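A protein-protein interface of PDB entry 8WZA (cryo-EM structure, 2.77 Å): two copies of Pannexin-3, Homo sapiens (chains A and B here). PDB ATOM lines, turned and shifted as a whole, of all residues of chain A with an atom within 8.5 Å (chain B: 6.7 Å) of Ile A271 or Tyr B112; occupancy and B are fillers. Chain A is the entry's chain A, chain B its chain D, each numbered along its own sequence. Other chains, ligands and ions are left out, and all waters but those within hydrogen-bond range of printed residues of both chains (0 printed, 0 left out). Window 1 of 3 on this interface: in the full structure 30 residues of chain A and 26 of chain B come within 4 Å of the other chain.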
ATOM      1  N   LEU A  49      29.564  16.773 -22.406  1.00  0.00           N
ATOM      2  CA  LEU A  49      28.761  17.230 -23.537  1.00  0.00           C
ATOM      3  C   LEU A  49      29.150  16.503 -24.818  1.00  0.00           C
ATOM      4  O   LEU A  49      28.281  16.111 -25.607  1.00  0.00           O
ATOM      5  CB  LEU A  49      28.907  18.742 -23.712  1.00  0.00           C
ATOM      6  CG  LEU A  49      28.108  19.622 -22.749  1.00  0.00           C
ATOM      7  CD1 LEU A  49      28.354  21.094 -23.041  1.00  0.00           C
ATOM      8  CD2 LEU A  49      26.626  19.297 -22.830  1.00  0.00           C
ATOM      9  N   LEU A  52      27.787  12.896 -24.619  1.00  0.00           N
ATOM     10  CA  LEU A  52      26.343  12.836 -24.826  1.00  0.00           C
ATOM     11  C   LEU A  52      25.958  13.142 -26.268  1.00  0.00           C
ATOM     12  O   LEU A  52      25.043  12.512 -26.810  1.00  0.00           O
ATOM     13  CB  LEU A  52      25.635  13.811 -23.884  1.00  0.00           C
ATOM     14  CG  LEU A  52      25.407  13.377 -22.437  1.00  0.00           C
ATOM     15  CD1 LEU A  52      25.021  14.575 -21.589  1.00  0.00           C
ATOM     16  CD2 LEU A  52      24.331  12.307 -22.371  1.00  0.00           C
ATOM     17  N   ALA A  53      26.638  14.100 -26.901  1.00  0.00           N
ATOM     18  CA  ALA A  53      26.179  14.602 -28.191  1.00  0.00           C
ATOM     19  C   ALA A  53      26.462  13.620 -29.322  1.00  0.00           C
ATOM     20  O   ALA A  53      25.685  13.531 -30.279  1.00  0.00           O
ATOM     21  CB  ALA A  53      26.829  15.955 -28.480  1.00  0.00           C
ATOM     22  N   ALA A  55      27.331  10.110 -29.037  1.00  0.00           N
ATOM     23  CA  ALA A  55      27.328   8.709 -28.632  1.00  0.00           C
ATOM     24  C   ALA A  55      26.038   8.433 -27.867  1.00  0.00           C
ATOM     25  O   ALA A  55      25.136   9.275 -27.812  1.00  0.00           O
ATOM     26  CB  ALA A  55      28.567   8.372 -27.796  1.00  0.00           C
ATOM     27  N   GLU A  57      22.798   8.060 -26.456  1.00  0.00           N
ATOM     28  CA  GLU A  57      21.363   8.195 -26.683  1.00  0.00           C
ATOM     29  C   GLU A  57      21.042   8.486 -28.144  1.00  0.00           C
ATOM     30  O   GLU A  57      20.311   7.731 -28.794  1.00  0.00           O
ATOM     31  CB  GLU A  57      20.820   9.290 -25.763  1.00  0.00           C
ATOM     32  CG  GLU A  57      21.802  10.438 -25.582  1.00  0.00           C
ATOM     33  CD  GLU A  57      21.494  11.298 -24.377  1.00  0.00           C
ATOM     34  OE1 GLU A  57      21.287  12.513 -24.553  1.00  0.00           O
ATOM     35  OE2 GLU A  57      21.455  10.759 -23.252  1.00  0.00           O
ATOM     36  N   PHE A  58      21.577   9.580 -28.682  1.00  0.00           N
ATOM     37  CA  PHE A  58      21.216  10.026 -30.027  1.00  0.00           C
ATOM     38  C   PHE A  58      22.228   9.476 -31.024  1.00  0.00           C
ATOM     39  O   PHE A  58      23.273  10.076 -31.283  1.00  0.00           O
ATOM     40  CB  PHE A  58      21.135  11.546 -30.086  1.00  0.00           C
ATOM     41  CG  PHE A  58      19.736  12.074 -29.998  1.00  0.00           C
ATOM     42  CD1 PHE A  58      18.923  11.738 -28.928  1.00  0.00           C
ATOM     43  CD2 PHE A  58      19.227  12.895 -30.989  1.00  0.00           C
ATOM     44  CE1 PHE A  58      17.634  12.217 -28.845  1.00  0.00           C
ATOM     45  CE2 PHE A  58      17.938  13.376 -30.910  1.00  0.00           C
ATOM     46  CZ  PHE A  58      17.142  13.035 -29.838  1.00  0.00           C
ATOM     47  N   SER A  59      21.909   8.316 -31.589  1.00  0.00           N
ATOM     48  CA  SER A  59      22.701   7.736 -32.670  1.00  0.00           C
ATOM     49  C   SER A  59      22.387   8.501 -33.948  1.00  0.00           C
ATOM     50  O   SER A  59      21.355   8.277 -34.584  1.00  0.00           O
ATOM     51  CB  SER A  59      22.396   6.250 -32.820  1.00  0.00           C
ATOM     52  OG  SER A  59      23.459   5.575 -33.469  1.00  0.00           O
ATOM     53  N   LEU A 110      32.150  21.180 -34.174  1.00  0.00           N
ATOM     54  CA  LEU A 110      31.747  21.170 -32.766  1.00  0.00           C
ATOM     55  C   LEU A 110      32.532  20.192 -31.894  1.00  0.00           C
ATOM     56  O   LEU A 110      33.000  20.606 -30.817  1.00  0.00           O
ATOM     57  CB  LEU A 110      30.237  20.910 -32.682  1.00  0.00           C
ATOM     58  CG  LEU A 110      29.550  21.154 -31.339  1.00  0.00           C
ATOM     59  CD1 LEU A 110      29.092  22.598 -31.233  1.00  0.00           C
ATOM     60  CD2 LEU A 110      28.376  20.206 -31.163  1.00  0.00           C
ATOM     61  N   HIS A 231      28.523  30.680 -33.571  1.00  0.00           N
ATOM     62  CA  HIS A 231      27.158  30.225 -33.340  1.00  0.00           C
ATOM     63  C   HIS A 231      26.234  31.441 -33.374  1.00  0.00           C
ATOM     64  O   HIS A 231      26.637  32.544 -33.758  1.00  0.00           O
ATOM     65  CB  HIS A 231      27.050  29.465 -32.020  1.00  0.00           C
ATOM     66  CG  HIS A 231      27.808  28.173 -31.988  1.00  0.00           C
ATOM     67  ND1 HIS A 231      28.965  27.963 -32.708  1.00  0.00           N
ATOM     68  CD2 HIS A 231      27.572  27.022 -31.314  1.00  0.00           C
ATOM     69  CE1 HIS A 231      29.408  26.740 -32.480  1.00  0.00           C
ATOM     70  NE2 HIS A 231      28.580  26.147 -31.639  1.00  0.00           N
ATOM     71  N   PHE A 235      21.871  29.185 -36.204  1.00  0.00           N
ATOM     72  CA  PHE A 235      21.207  28.636 -35.028  1.00  0.00           C
ATOM     73  C   PHE A 235      19.791  28.171 -35.312  1.00  0.00           C
ATOM     74  O   PHE A 235      19.350  27.167 -34.749  1.00  0.00           O
ATOM     75  CB  PHE A 235      21.184  29.671 -33.891  1.00  0.00           C
ATOM     76  CG  PHE A 235      20.911  29.080 -32.533  1.00  0.00           C
ATOM     77  CD1 PHE A 235      21.914  28.435 -31.828  1.00  0.00           C
ATOM     78  CD2 PHE A 235      19.651  29.168 -31.964  1.00  0.00           C
ATOM     79  CE1 PHE A 235      21.666  27.891 -30.581  1.00  0.00           C
ATOM     80  CE2 PHE A 235      19.396  28.625 -30.717  1.00  0.00           C
ATOM     81  CZ  PHE A 235      20.406  27.986 -30.026  1.00  0.00           C
ATOM     82  N   SER A 265      21.083  17.061 -37.011  1.00  0.00           N
ATOM     83  CA  SER A 265      21.467  17.211 -35.607  1.00  0.00           C
ATOM     84  C   SER A 265      21.424  18.661 -35.135  1.00  0.00           C
ATOM     85  O   SER A 265      22.274  19.084 -34.347  1.00  0.00           O
ATOM     86  CB  SER A 265      22.854  16.619 -35.379  1.00  0.00           C
ATOM     87  OG  SER A 265      22.888  15.248 -35.735  1.00  0.00           O
ATOM     88  N   LEU A 266      20.452  19.448 -35.602  1.00  0.00           N
ATOM     89  CA  LEU A 266      20.367  20.844 -35.179  1.00  0.00           C
ATOM     90  C   LEU A 266      19.981  20.963 -33.707  1.00  0.00           C
ATOM     91  O   LEU A 266      20.458  21.863 -33.003  1.00  0.00           O
ATOM     92  CB  LEU A 266      19.369  21.596 -36.057  1.00  0.00           C
ATOM     93  CG  LEU A 266      19.276  23.108 -35.840  1.00  0.00           C
ATOM     94  CD1 LEU A 266      20.570  23.787 -36.259  1.00  0.00           C
ATOM     95  CD2 LEU A 266      18.091  23.692 -36.590  1.00  0.00           C
ATOM     96  N   SER A 267      19.114  20.068 -33.226  1.00  0.00           N
ATOM     97  CA  SER A 267      18.676  20.131 -31.834  1.00  0.00           C
ATOM     98  C   SER A 267      19.834  19.889 -30.874  1.00  0.00           C
ATOM     99  O   SER A 267      19.949  20.566 -29.845  1.00  0.00           O
ATOM    100  CB  SER A 267      17.556  19.117 -31.593  1.00  0.00           C
ATOM    101  OG  SER A 267      16.411  19.431 -32.365  1.00  0.00           O
ATOM    102  N   ILE A 268      20.700  18.925 -31.194  1.00  0.00           N
ATOM    103  CA  ILE A 268      21.882  18.679 -30.372  1.00  0.00           C
ATOM    104  C   ILE A 268      22.788  19.902 -30.373  1.00  0.00           C
ATOM    105  O   ILE A 268      23.341  20.287 -29.336  1.00  0.00           O
ATOM    106  CB  ILE A 268      22.623  17.424 -30.869  1.00  0.00           C
ATOM    107  CG1 ILE A 268      21.757  16.178 -30.677  1.00  0.00           C
ATOM    108  CG2 ILE A 268      23.950  17.265 -30.150  1.00  0.00           C
ATOM    109  CD1 ILE A 268      21.388  15.493 -31.973  1.00  0.00           C
ATOM    110  N   PHE A 269      22.956  20.527 -31.541  1.00  0.00           N
ATOM    111  CA  PHE A 269      23.728  21.761 -31.648  1.00  0.00           C
ATOM    112  C   PHE A 269      23.201  22.822 -30.687  1.00  0.00           C
ATOM    113  O   PHE A 269      23.958  23.388 -29.883  1.00  0.00           O
ATOM    114  CB  PHE A 269      23.665  22.251 -33.098  1.00  0.00           C
ATOM    115  CG  PHE A 269      24.651  23.331 -33.436  1.00  0.00           C
ATOM    116  CD1 PHE A 269      25.986  23.031 -33.642  1.00  0.00           C
ATOM    117  CD2 PHE A 269      24.231  24.641 -33.593  1.00  0.00           C
ATOM    118  CE1 PHE A 269      26.889  24.024 -33.970  1.00  0.00           C
ATOM    119  CE2 PHE A 269      25.128  25.636 -33.920  1.00  0.00           C
ATOM    120  CZ  PHE A 269      26.458  25.328 -34.110  1.00  0.00           C
ATOM    121  N   GLN A 270      21.891  23.081 -30.740  1.00  0.00           N
ATOM    122  CA  GLN A 270      21.294  24.114 -29.899  1.00  0.00           C
ATOM    123  C   GLN A 270      21.433  23.781 -28.418  1.00  0.00           C
ATOM    124  O   GLN A 270      21.780  24.651 -27.606  1.00  0.00           O
ATOM    125  CB  GLN A 270      19.821  24.292 -30.272  1.00  0.00           C
ATOM    126  CG  GLN A 270      19.596  24.834 -31.675  1.00  0.00           C
ATOM    127  CD  GLN A 270      18.161  24.681 -32.137  1.00  0.00           C
ATOM    128  OE1 GLN A 270      17.408  23.867 -31.603  1.00  0.00           O
ATOM    129  NE2 GLN A 270      17.774  25.462 -33.139  1.00  0.00           N
ATOM    130  N   ILE A 271      21.172  22.526 -28.048  1.00  0.00           N
ATOM    131  CA  ILE A 271      21.211  22.140 -26.640  1.00  0.00           C
ATOM    132  C   ILE A 271      22.631  22.237 -26.096  1.00  0.00           C
ATOM    133  O   ILE A 271      22.851  22.722 -24.978  1.00  0.00           O
ATOM    134  CB  ILE A 271      20.618  20.730 -26.460  1.00  0.00           C
ATOM    135  CG1 ILE A 271      19.091  20.807 -26.457  1.00  0.00           C
ATOM    136  CG2 ILE A 271      21.123  20.085 -25.178  1.00  0.00           C
ATOM    137  CD1 ILE A 271      18.412  19.493 -26.726  1.00  0.00           C
ATOM    138  N   VAL A 272      23.615  21.784 -26.877  1.00  0.00           N
ATOM    139  CA  VAL A 272      25.007  21.866 -26.445  1.00  0.00           C
ATOM    140  C   VAL A 272      25.423  23.320 -26.269  1.00  0.00           C
ATOM    141  O   VAL A 272      26.077  23.677 -25.279  1.00  0.00           O
ATOM    142  CB  VAL A 272      25.919  21.125 -27.441  1.00  0.00           C
ATOM    143  CG1 VAL A 272      27.350  21.630 -27.343  1.00  0.00           C
ATOM    144  CG2 VAL A 272      25.861  19.624 -27.195  1.00  0.00           C
ATOM    145  N   SER A 273      25.044  24.186 -27.215  1.00  0.00           N
ATOM    146  CA  SER A 273      25.399  25.599 -27.095  1.00  0.00           C
ATOM    147  C   SER A 273      24.792  26.218 -25.840  1.00  0.00           C
ATOM    148  O   SER A 273      25.472  26.931 -25.088  1.00  0.00           O
ATOM    149  CB  SER A 273      24.946  26.354 -28.345  1.00  0.00           C
ATOM    150  OG  SER A 273      24.935  27.754 -28.122  1.00  0.00           O
ATOM    151  N   LEU A 274      23.508  25.941 -25.586  1.00  0.00           N
ATOM    152  CA  LEU A 274      22.848  26.521 -24.420  1.00  0.00           C
ATOM    153  C   LEU A 274      23.460  26.014 -23.118  1.00  0.00           C
ATOM    154  O   LEU A 274      23.669  26.794 -22.179  1.00  0.00           O
ATOM    155  CB  LEU A 274      21.349  26.227 -24.465  1.00  0.00           C
ATOM    156  CG  LEU A 274      20.536  27.076 -25.445  1.00  0.00           C
ATOM    157  CD1 LEU A 274      19.052  26.994 -25.128  1.00  0.00           C
ATOM    158  CD2 LEU A 274      21.012  28.521 -25.434  1.00  0.00           C
ATOM    159  N   SER A 275      23.751  24.712 -23.039  1.00  0.00           N
ATOM    160  CA  SER A 275      24.370  24.168 -21.834  1.00  0.00           C
ATOM    161  C   SER A 275      25.752  24.767 -21.606  1.00  0.00           C
ATOM    162  O   SER A 275      26.122  25.081 -20.466  1.00  0.00           O
ATOM    163  CB  SER A 275      24.455  22.644 -21.931  1.00  0.00           C
ATOM    164  OG  SER A 275      23.219  22.089 -22.346  1.00  0.00           O
ATOM    165  N   SER A 276      26.530  24.928 -22.682  1.00  0.00           N
ATOM    166  CA  SER A 276      27.854  25.529 -22.556  1.00  0.00           C
ATOM    167  C   SER A 276      27.762  26.957 -22.040  1.00  0.00           C
ATOM    168  O   SER A 276      28.572  27.376 -21.205  1.00  0.00           O
ATOM    169  CB  SER A 276      28.576  25.491 -23.903  1.00  0.00           C
ATOM    170  OG  SER A 276      29.023  24.181 -24.205  1.00  0.00           O
ATOM    171  N   VAL A 277      26.784  27.724 -22.527  1.00  0.00           N
ATOM    172  CA  VAL A 277      26.602  29.085 -22.024  1.00  0.00           C
ATOM    173  C   VAL A 277      26.247  29.059 -20.539  1.00  0.00           C
ATOM    174  O   VAL A 277      26.857  29.763 -19.720  1.00  0.00           O
ATOM    175  CB  VAL A 277      25.531  29.825 -22.846  1.00  0.00           C
ATOM    176  CG1 VAL A 277      24.980  31.010 -22.064  1.00  0.00           C
ATOM    177  CG2 VAL A 277      26.103  30.282 -24.176  1.00  0.00           C
ATOM    178  N   ALA A 278      25.262  28.232 -20.172  1.00  0.00           N
ATOM    179  CA  ALA A 278      24.723  28.263 -18.816  1.00  0.00           C
ATOM    180  C   ALA A 278      25.756  27.832 -17.780  1.00  0.00           C
ATOM    181  O   ALA A 278      25.869  28.454 -16.716  1.00  0.00           O
ATOM    182  CB  ALA A 278      23.480  27.379 -18.727  1.00  0.00           C
ATOM    183  N   ILE A 279      26.512  26.768 -18.066  1.00  0.00           N
ATOM    184  CA  ILE A 279      27.443  26.237 -17.072  1.00  0.00           C
ATOM    185  C   ILE A 279      28.515  27.269 -16.739  1.00  0.00           C
ATOM    186  O   ILE A 279      28.821  27.522 -15.566  1.00  0.00           O
ATOM    187  CB  ILE A 279      28.057  24.913 -17.563  1.00  0.00           C
ATOM    188  CG1 ILE A 279      27.130  23.745 -17.223  1.00  0.00           C
ATOM    189  CG2 ILE A 279      29.431  24.691 -16.947  1.00  0.00           C
ATOM    190  CD1 ILE A 279      27.178  22.612 -18.225  1.00  0.00           C
ATOM    191  N   MET B  50      16.359   5.316 -17.309  1.00  0.00           N
ATOM    192  CA  MET B  50      17.040   5.655 -18.554  1.00  0.00           C
ATOM    193  C   MET B  50      17.698   4.430 -19.176  1.00  0.00           C
ATOM    194  O   MET B  50      17.647   4.241 -20.397  1.00  0.00           O
ATOM    195  CB  MET B  50      18.074   6.752 -18.298  1.00  0.00           C
ATOM    196  CG  MET B  50      19.052   6.976 -19.440  1.00  0.00           C
ATOM    197  SD  MET B  50      20.369   8.146 -19.042  1.00  0.00           S
ATOM    198  CE  MET B  50      19.851   8.734 -17.430  1.00  0.00           C
ATOM    199  N   PHE B  54      16.105   3.028 -23.011  1.00  0.00           N
ATOM    200  CA  PHE B  54      16.866   3.281 -24.230  1.00  0.00           C
ATOM    201  C   PHE B  54      18.016   2.295 -24.410  1.00  0.00           C
ATOM    202  O   PHE B  54      19.054   2.641 -24.976  1.00  0.00           O
ATOM    203  CB  PHE B  54      17.382   4.719 -24.246  1.00  0.00           C
ATOM    204  CG  PHE B  54      16.321   5.741 -23.953  1.00  0.00           C
ATOM    205  CD1 PHE B  54      16.144   6.230 -22.669  1.00  0.00           C
ATOM    206  CD2 PHE B  54      15.486   6.197 -24.960  1.00  0.00           C
ATOM    207  CE1 PHE B  54      15.163   7.164 -22.399  1.00  0.00           C
ATOM    208  CE2 PHE B  54      14.503   7.129 -24.695  1.00  0.00           C
ATOM    209  CZ  PHE B  54      14.341   7.613 -23.413  1.00  0.00           C
ATOM    210  N   LYS B 108      11.419  13.736 -27.536  1.00  0.00           N
ATOM    211  CA  LYS B 108      12.831  13.864 -27.866  1.00  0.00           C
ATOM    212  C   LYS B 108      13.685  14.184 -26.644  1.00  0.00           C
ATOM    213  O   LYS B 108      14.867  13.824 -26.610  1.00  0.00           O
ATOM    214  CB  LYS B 108      13.020  14.942 -28.937  1.00  0.00           C
ATOM    215  CG  LYS B 108      14.238  14.726 -29.817  1.00  0.00           C
ATOM    216  CD  LYS B 108      14.576  15.943 -30.667  1.00  0.00           C
ATOM    217  CE  LYS B 108      13.336  16.715 -31.082  1.00  0.00           C
ATOM    218  NZ  LYS B 108      13.665  17.817 -32.028  1.00  0.00           N
ATOM    219  N   ALA B 109      13.116  14.852 -25.640  1.00  0.00           N
ATOM    220  CA  ALA B 109      13.892  15.345 -24.508  1.00  0.00           C
ATOM    221  C   ALA B 109      13.921  14.401 -23.311  1.00  0.00           C
ATOM    222  O   ALA B 109      14.638  14.685 -22.346  1.00  0.00           O
ATOM    223  CB  ALA B 109      13.353  16.706 -24.056  1.00  0.00           C
ATOM    224  N   LEU B 110      13.165  13.300 -23.343  1.00  0.00           N
ATOM    225  CA  LEU B 110      13.044  12.444 -22.161  1.00  0.00           C
ATOM    226  C   LEU B 110      14.379  11.979 -21.577  1.00  0.00           C
ATOM    227  O   LEU B 110      14.565  12.111 -20.353  1.00  0.00           O
ATOM    228  CB  LEU B 110      12.136  11.254 -22.496  1.00  0.00           C
ATOM    229  CG  LEU B 110      11.646  10.388 -21.335  1.00  0.00           C
ATOM    230  CD1 LEU B 110      10.349  10.940 -20.770  1.00  0.00           C
ATOM    231  CD2 LEU B 110      11.461   8.949 -21.786  1.00  0.00           C
ATOM    232  N   PRO B 111      15.326  11.422 -22.347  1.00  0.00           N
ATOM    233  CA  PRO B 111      16.605  11.025 -21.722  1.00  0.00           C
ATOM    234  C   PRO B 111      17.377  12.193 -21.130  1.00  0.00           C
ATOM    235  O   PRO B 111      17.997  12.051 -20.063  1.00  0.00           O
ATOM    236  CB  PRO B 111      17.369  10.357 -22.875  1.00  0.00           C
ATOM    237  CG  PRO B 111      16.732  10.873 -24.114  1.00  0.00           C
ATOM    238  CD  PRO B 111      15.291  11.067 -23.778  1.00  0.00           C
ATOM    239  N   TYR B 112      17.343  13.354 -21.792  1.00  0.00           N
ATOM    240  CA  TYR B 112      17.991  14.540 -21.240  1.00  0.00           C
ATOM    241  C   TYR B 112      17.392  14.894 -19.889  1.00  0.00           C
ATOM    242  O   TYR B 112      18.117  15.200 -18.936  1.00  0.00           O
ATOM    243  CB  TYR B 112      17.844  15.738 -22.185  1.00  0.00           C
ATOM    244  CG  TYR B 112      18.108  15.507 -23.662  1.00  0.00           C
ATOM    245  CD1 TYR B 112      17.593  16.384 -24.609  1.00  0.00           C
ATOM    246  CD2 TYR B 112      18.887  14.451 -24.112  1.00  0.00           C
ATOM    247  CE1 TYR B 112      17.821  16.201 -25.957  1.00  0.00           C
ATOM    248  CE2 TYR B 112      19.119  14.262 -25.465  1.00  0.00           C
ATOM    249  CZ  TYR B 112      18.587  15.141 -26.380  1.00  0.00           C
ATOM    250  OH  TYR B 112      18.820  14.960 -27.724  1.00  0.00           O
ATOM    251  N   SER B 113      16.060  14.860 -19.796  1.00  0.00           N
ATOM    252  CA  SER B 113      15.386  15.198 -18.550  1.00  0.00           C
ATOM    253  C   SER B 113      15.715  14.196 -17.452  1.00  0.00           C
ATOM    254  O   SER B 113      15.896  14.578 -16.290  1.00  0.00           O
ATOM    255  CB  SER B 113      13.876  15.267 -18.779  1.00  0.00           C
ATOM    256  OG  SER B 113      13.522  16.451 -19.472  1.00  0.00           O
ATOM    257  N   LEU B 114      15.789  12.908 -17.796  1.00  0.00           N
ATOM    258  CA  LEU B 114      16.142  11.908 -16.792  1.00  0.00           C
ATOM    259  C   LEU B 114      17.552  12.137 -16.257  1.00  0.00           C
ATOM    260  O   LEU B 114      17.782  12.082 -15.040  1.00  0.00           O
ATOM    261  CB  LEU B 114      16.007  10.503 -17.377  1.00  0.00           C
ATOM    262  CG  LEU B 114      14.573   9.985 -17.516  1.00  0.00           C
ATOM    263  CD1 LEU B 114      14.551   8.611 -18.167  1.00  0.00           C
ATOM    264  CD2 LEU B 114      13.878   9.954 -16.164  1.00  0.00           C
ATOM    265  N   LEU B 115      18.508  12.415 -17.149  1.00  0.00           N
ATOM    266  CA  LEU B 115      19.869  12.692 -16.695  1.00  0.00           C
ATOM    267  C   LEU B 115      19.922  13.957 -15.845  1.00  0.00           C
ATOM    268  O   LEU B 115      20.630  14.004 -14.829  1.00  0.00           O
ATOM    269  CB  LEU B 115      20.813  12.808 -17.892  1.00  0.00           C
ATOM    270  CG  LEU B 115      22.304  12.795 -17.548  1.00  0.00           C
ATOM    271  CD1 LEU B 115      22.736  11.418 -17.069  1.00  0.00           C
ATOM    272  CD2 LEU B 115      23.137  13.235 -18.739  1.00  0.00           C
ATOM    273  N   ALA B 116      19.182  14.993 -16.247  1.00  0.00           N
ATOM    274  CA  ALA B 116      19.161  16.233 -15.478  1.00  0.00           C
ATOM    275  C   ALA B 116      18.580  16.012 -14.088  1.00  0.00           C
ATOM    276  O   ALA B 116      19.084  16.564 -13.105  1.00  0.00           O
ATOM    277  CB  ALA B 116      18.369  17.302 -16.228  1.00  0.00           C
ATOM    278  N   LEU B 117      17.514  15.214 -13.986  1.00  0.00           N
ATOM    279  CA  LEU B 117      16.932  14.915 -12.681  1.00  0.00           C
ATOM    280  C   LEU B 117      17.903  14.128 -11.808  1.00  0.00           C
ATOM    281  O   LEU B 117      18.020  14.388 -10.603  1.00  0.00           O
ATOM    282  CB  LEU B 117      15.623  14.145 -12.859  1.00  0.00           C
ATOM    283  CG  LEU B 117      14.876  13.743 -11.586  1.00  0.00           C
ATOM    284  CD1 LEU B 117      14.520  14.968 -10.761  1.00  0.00           C
ATOM    285  CD2 LEU B 117      13.630  12.944 -11.931  1.00  0.00           C
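Leu B115 touches Leu A52 (CD2 to CD1, 3.7 Å). Glu A57 touches Tyr B112 (OE1 to CE2, 2.9 Å). Phe A58 touches Lys B108. CE1 of Phe A58 touches OH of Tyr B112 (3.2 Å). CD1 of Ile A271 touches CE1 of Tyr B112 (3.4 Å).
1 position is printed for both chains.
The side-chain amino group (NZ) of Lys B108 lies within hydrogen-bond range of the side-chain hydroxyl (OG) of Ser A267 (3.2 Å).
Along chain B the printed residues that touch a printed residue of chain A span positions 108 to 115. Hydrophobic or aromatic side chains of chain A that line the printed part of chain B: Leu A52, Phe A58 and Ile A271. Among the printed residues, no Asp or Glu carboxylate lies within 4 Å of a Lys or Arg side-chain nitrogen of the other chain.
Of the printed residues of chain B, Ile A271 touches Tyr B112. Of chain A, only Glu A57 (2.9 Å), Phe A58 (3.2 Å) and Ile A271 (3.4 Å) come within 4 Å of Tyr B112. Pro B111 touches none of the printed residues of chain A. No residue of chain A comes within 4 Å of Ser B113. Of the printed residues of chain B, Ser A267 touches Lys B108. Of the printed residues of chain B, Phe A58 touches Lys B108 (3.4 Å) and Tyr B112 (3.2 Å). Of the printed residues of chain A, Leu B115 touches Leu A52 (3.7 Å). Leu A49 touches none of the printed residues of chain B. The nearest residue of chain A that does not touch Tyr B112 is Ile A268 (4.3 Å).
The side-chain hydroxyl (OG) of Ser A275 lies within hydrogen-bond range of the backbone carbonyl oxygen (O) of Ile A271 (2.7 Å).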
